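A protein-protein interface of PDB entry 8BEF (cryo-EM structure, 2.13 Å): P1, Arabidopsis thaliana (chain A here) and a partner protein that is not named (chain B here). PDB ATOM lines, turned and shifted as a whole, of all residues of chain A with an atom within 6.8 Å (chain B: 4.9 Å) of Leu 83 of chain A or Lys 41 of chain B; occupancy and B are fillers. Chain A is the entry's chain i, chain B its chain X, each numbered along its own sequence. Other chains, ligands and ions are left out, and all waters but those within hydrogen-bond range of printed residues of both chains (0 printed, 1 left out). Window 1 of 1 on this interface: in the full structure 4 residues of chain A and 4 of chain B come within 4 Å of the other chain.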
ATOM      1  N   ASP A  77       7.661  30.555  -3.646  1.00  0.00           N
ATOM      2  CA  ASP A  77       6.892  29.540  -2.942  1.00  0.00           C
ATOM      3  C   ASP A  77       7.431  29.431  -1.519  1.00  0.00           C
ATOM      4  O   ASP A  77       8.653  29.391  -1.329  1.00  0.00           O
ATOM      5  CB  ASP A  77       6.994  28.195  -3.671  1.00  0.00           C
ATOM      6  CG  ASP A  77       6.131  27.099  -3.043  1.00  0.00           C
ATOM      7  OD1 ASP A  77       5.426  27.356  -2.049  1.00  0.00           O
ATOM      8  OD2 ASP A  77       6.144  25.966  -3.559  1.00  0.00           O
ATOM      9  N   PRO A  78       6.567  29.399  -0.499  1.00  0.00           N
ATOM     10  CA  PRO A  78       7.072  29.367   0.884  1.00  0.00           C
ATOM     11  C   PRO A  78       7.979  28.185   1.185  1.00  0.00           C
ATOM     12  O   PRO A  78       8.855  28.302   2.051  1.00  0.00           O
ATOM     13  CB  PRO A  78       5.787  29.326   1.727  1.00  0.00           C
ATOM     14  CG  PRO A  78       4.681  29.004   0.770  1.00  0.00           C
ATOM     15  CD  PRO A  78       5.107  29.562  -0.544  1.00  0.00           C
ATOM     16  N   TYR A  79       7.817  27.058   0.491  1.00  0.00           N
ATOM     17  CA  TYR A  79       8.655  25.897   0.766  1.00  0.00           C
ATOM     18  C   TYR A  79      10.079  26.048   0.237  1.00  0.00           C
ATOM     19  O   TYR A  79      10.959  25.293   0.657  1.00  0.00           O
ATOM     20  CB  TYR A  79       8.005  24.640   0.190  1.00  0.00           C
ATOM     21  CG  TYR A  79       6.836  24.167   1.018  1.00  0.00           C
ATOM     22  CD1 TYR A  79       7.029  23.700   2.311  1.00  0.00           C
ATOM     23  CD2 TYR A  79       5.541  24.211   0.521  1.00  0.00           C
ATOM     24  CE1 TYR A  79       5.968  23.277   3.081  1.00  0.00           C
ATOM     25  CE2 TYR A  79       4.474  23.790   1.286  1.00  0.00           C
ATOM     26  CZ  TYR A  79       4.694  23.324   2.564  1.00  0.00           C
ATOM     27  OH  TYR A  79       3.638  22.901   3.333  1.00  0.00           O
ATOM     28  N   ASP A  80      10.328  26.999  -0.669  1.00  0.00           N
ATOM     29  CA  ASP A  80      11.686  27.212  -1.166  1.00  0.00           C
ATOM     30  C   ASP A  80      12.631  27.670  -0.065  1.00  0.00           C
ATOM     31  O   ASP A  80      13.814  27.314  -0.075  1.00  0.00           O
ATOM     32  CB  ASP A  80      11.680  28.230  -2.306  1.00  0.00           C
ATOM     33  CG  ASP A  80      10.555  28.001  -3.281  1.00  0.00           C
ATOM     34  OD1 ASP A  80      10.015  26.879  -3.296  1.00  0.00           O
ATOM     35  OD2 ASP A  80      10.202  28.938  -4.025  1.00  0.00           O
ATOM     36  N   ASP A  81      12.138  28.463   0.885  1.00  0.00           N
ATOM     37  CA  ASP A  81      12.990  28.919   1.976  1.00  0.00           C
ATOM     38  C   ASP A  81      13.324  27.778   2.931  1.00  0.00           C
ATOM     39  O   ASP A  81      14.435  27.720   3.469  1.00  0.00           O
ATOM     40  CB  ASP A  81      12.318  30.072   2.717  1.00  0.00           C
ATOM     41  CG  ASP A  81      13.261  31.230   2.967  1.00  0.00           C
ATOM     42  OD1 ASP A  81      14.486  31.046   2.804  1.00  0.00           O
ATOM     43  OD2 ASP A  81      12.780  32.325   3.328  1.00  0.00           O
ATOM     44  N   LEU A  82      12.377  26.864   3.156  1.00  0.00           N
ATOM     45  CA  LEU A  82      12.618  25.740   4.055  1.00  0.00           C
ATOM     46  C   LEU A  82      13.675  24.783   3.525  1.00  0.00           C
ATOM     47  O   LEU A  82      14.370  24.145   4.321  1.00  0.00           O
ATOM     48  CB  LEU A  82      11.323  24.963   4.308  1.00  0.00           C
ATOM     49  CG  LEU A  82      10.299  25.535   5.289  1.00  0.00           C
ATOM     50  CD1 LEU A  82      10.998  26.093   6.507  1.00  0.00           C
ATOM     51  CD2 LEU A  82       9.427  26.588   4.648  1.00  0.00           C
ATOM     52  N   LEU A  83      13.808  24.663   2.207  1.00  0.00           N
ATOM     53  CA  LEU A  83      14.744  23.720   1.615  1.00  0.00           C
ATOM     54  C   LEU A  83      16.028  24.372   1.127  1.00  0.00           C
ATOM     55  O   LEU A  83      16.964  23.654   0.762  1.00  0.00           O
ATOM     56  CB  LEU A  83      14.072  22.976   0.459  1.00  0.00           C
ATOM     57  CG  LEU A  83      13.153  21.853   0.940  1.00  0.00           C
ATOM     58  CD1 LEU A  83      12.589  21.057  -0.222  1.00  0.00           C
ATOM     59  CD2 LEU A  83      13.902  20.946   1.897  1.00  0.00           C
ATOM     60  N   GLU A  84      16.104  25.699   1.121  1.00  0.00           N
ATOM     61  CA  GLU A  84      17.316  26.389   0.693  1.00  0.00           C
ATOM     62  C   GLU A  84      17.987  27.090   1.869  1.00  0.00           C
ATOM     63  O   GLU A  84      19.210  27.227   1.907  1.00  0.00           O
ATOM     64  CB  GLU A  84      16.998  27.400  -0.411  1.00  0.00           C
ATOM     65  CG  GLU A  84      16.993  26.812  -1.814  1.00  0.00           C
ATOM     66  CD  GLU A  84      18.388  26.530  -2.335  1.00  0.00           C
ATOM     67  OE1 GLU A  84      19.315  27.299  -2.003  1.00  0.00           O
ATOM     68  OE2 GLU A  84      18.557  25.541  -3.079  1.00  0.00           O
ATOM     69  N   VAL B  34      13.777  17.026   6.169  1.00  0.00           N
ATOM     70  CA  VAL B  34      14.091  17.367   4.784  1.00  0.00           C
ATOM     71  C   VAL B  34      13.232  16.557   3.823  1.00  0.00           C
ATOM     72  O   VAL B  34      12.740  17.082   2.819  1.00  0.00           O
ATOM     73  CB  VAL B  34      15.594  17.174   4.512  1.00  0.00           C
ATOM     74  CG1 VAL B  34      15.904  17.415   3.045  1.00  0.00           C
ATOM     75  CG2 VAL B  34      16.407  18.104   5.384  1.00  0.00           C
ATOM     76  N   LEU B  37       9.751  17.974   3.764  1.00  0.00           N
ATOM     77  CA  LEU B  37       9.698  19.248   3.054  1.00  0.00           C
ATOM     78  C   LEU B  37       9.818  19.058   1.547  1.00  0.00           C
ATOM     79  O   LEU B  37       9.140  19.748   0.780  1.00  0.00           O
ATOM     80  CB  LEU B  37      10.780  20.191   3.575  1.00  0.00           C
ATOM     81  CG  LEU B  37      10.599  20.585   5.041  1.00  0.00           C
ATOM     82  CD1 LEU B  37      11.741  21.460   5.518  1.00  0.00           C
ATOM     83  CD2 LEU B  37       9.261  21.280   5.229  1.00  0.00           C
ATOM     84  N   LYS B  38      10.666  18.130   1.098  1.00  0.00           N
ATOM     85  CA  LYS B  38      10.729  17.829  -0.330  1.00  0.00           C
ATOM     86  C   LYS B  38       9.378  17.348  -0.843  1.00  0.00           C
ATOM     87  O   LYS B  38       8.888  17.819  -1.879  1.00  0.00           O
ATOM     88  CB  LYS B  38      11.808  16.782  -0.619  1.00  0.00           C
ATOM     89  CG  LYS B  38      13.204  17.158  -0.178  1.00  0.00           C
ATOM     90  CD  LYS B  38      14.250  16.609  -1.134  1.00  0.00           C
ATOM     91  CE  LYS B  38      15.490  16.152  -0.387  1.00  0.00           C
ATOM     92  NZ  LYS B  38      16.635  17.080  -0.586  1.00  0.00           N
ATOM     93  N   CYS B  39       8.747  16.420  -0.118  1.00  0.00           N
ATOM     94  CA  CYS B  39       7.478  15.882  -0.599  1.00  0.00           C
ATOM     95  C   CYS B  39       6.398  16.960  -0.611  1.00  0.00           C
ATOM     96  O   CYS B  39       5.580  17.016  -1.537  1.00  0.00           O
ATOM     97  CB  CYS B  39       7.049  14.685   0.249  1.00  0.00           C
ATOM     98  SG  CYS B  39       5.302  14.289   0.111  1.00  0.00           S
ATOM     99  N   LYS B  40       6.390  17.834   0.401  1.00  0.00           N
ATOM    100  CA  LYS B  40       5.462  18.961   0.408  1.00  0.00           C
ATOM    101  C   LYS B  40       5.727  19.901  -0.761  1.00  0.00           C
ATOM    102  O   LYS B  40       4.787  20.429  -1.366  1.00  0.00           O
ATOM    103  CB  LYS B  40       5.559  19.717   1.736  1.00  0.00           C
ATOM    104  CG  LYS B  40       4.855  19.042   2.903  1.00  0.00           C
ATOM    105  CD  LYS B  40       3.443  18.620   2.526  1.00  0.00           C
ATOM    106  CE  LYS B  40       2.490  19.800   2.517  1.00  0.00           C
ATOM    107  NZ  LYS B  40       1.167  19.447   3.099  1.00  0.00           N
ATOM    108  N   LYS B  41       7.003  20.128  -1.086  1.00  0.00           N
ATOM    109  CA  LYS B  41       7.348  20.940  -2.248  1.00  0.00           C
ATOM    110  C   LYS B  41       6.773  20.351  -3.527  1.00  0.00           C
ATOM    111  O   LYS B  41       6.241  21.082  -4.369  1.00  0.00           O
ATOM    112  CB  LYS B  41       8.866  21.070  -2.368  1.00  0.00           C
ATOM    113  CG  LYS B  41       9.326  22.291  -3.132  1.00  0.00           C
ATOM    114  CD  LYS B  41      10.753  22.658  -2.788  1.00  0.00           C
ATOM    115  CE  LYS B  41      11.419  23.410  -3.929  1.00  0.00           C
ATOM    116  NZ  LYS B  41      10.453  24.256  -4.678  1.00  0.00           N
ATOM    117  N   ASN B  42       6.879  19.033  -3.697  1.00  0.00           N
ATOM    118  CA  ASN B  42       6.349  18.420  -4.912  1.00  0.00           C
ATOM    119  C   ASN B  42       4.824  18.401  -4.905  1.00  0.00           C
ATOM    120  O   ASN B  42       4.190  18.630  -5.942  1.00  0.00           O
ATOM    121  CB  ASN B  42       6.928  17.010  -5.080  1.00  0.00           C
ATOM    122  CG  ASN B  42       6.541  16.356  -6.398  1.00  0.00           C
ATOM    123  OD1 ASN B  42       5.571  16.743  -7.049  1.00  0.00           O
ATOM    124  ND2 ASN B  42       7.308  15.348  -6.796  1.00  0.00           N
ATOM    125  N   ASP B  43       4.216  18.137  -3.753  1.00  0.00           N
ATOM    126  CA  ASP B  43       2.766  18.001  -3.705  1.00  0.00           C
ATOM    127  C   ASP B  43       2.185  18.604  -2.432  1.00  0.00           C
ATOM    128  O   ASP B  43       2.434  18.098  -1.331  1.00  0.00           O
ATOM    129  CB  ASP B  43       2.369  16.530  -3.816  1.00  0.00           C
ATOM    130  CG  ASP B  43       1.212  16.310  -4.766  1.00  0.00           C
ATOM    131  OD1 ASP B  43       0.332  17.189  -4.836  1.00  0.00           O
ATOM    132  OD2 ASP B  43       1.186  15.260  -5.439  1.00  0.00           O
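Leu 83 of chain A touches just these residues of chain B: Leu 37, Lys 38 and Lys 41.
Printed residues of chain B within 4 Å of Tyr 79 of chain A: Lys 40 (3.4 Å).
Of the printed residues of chain B, Leu 82 of chain A touches Leu 37 (3.7 Å).
Of the printed residues of chain A, Lys 38 of chain B touches Leu 83 (3.7 Å).
Pro 78 of chain A touches none of the printed residues of chain B.
The nearest printed residue of chain A that does not touch Leu 37 of chain B is Tyr 79 of chain A (4.4 Å).
CE of Lys 40 of chain B touches OH of Tyr 79 of chain A, at 3.4 Å.
CB of Leu 82 of chain A touches CD1 of Leu 37 of chain B, 3.7 Å away.
CD2 of Leu 83 of chain A touches CB of Leu 37 of chain B (3.6 Å).
Leu 83 of chain A touches Lys 38 of chain B.
Leu 83 of chain A touches Lys 41 of chain B (CD1 to CD, 3.5 Å).
The backbone NH of Asp 77 of chain A sits at hydrogen-bond distance from the side-chain carboxylate of Asp 80 of chain A.
Hydrophobic or aromatic side chains of chain B that line the printed part of chain A: Leu 37.
Of the 8 printed residues of chain A, 4 touch a printed residue of chain B.
Hydrophobic or aromatic side chains of chain A within 4 Å of the printed part of chain B: Tyr 79, Leu 82 and Leu 83.
OD1 of Asp 80 of chain A is in salt-bridge range of NZ of Lys 41 of chain B (3.0 Å).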
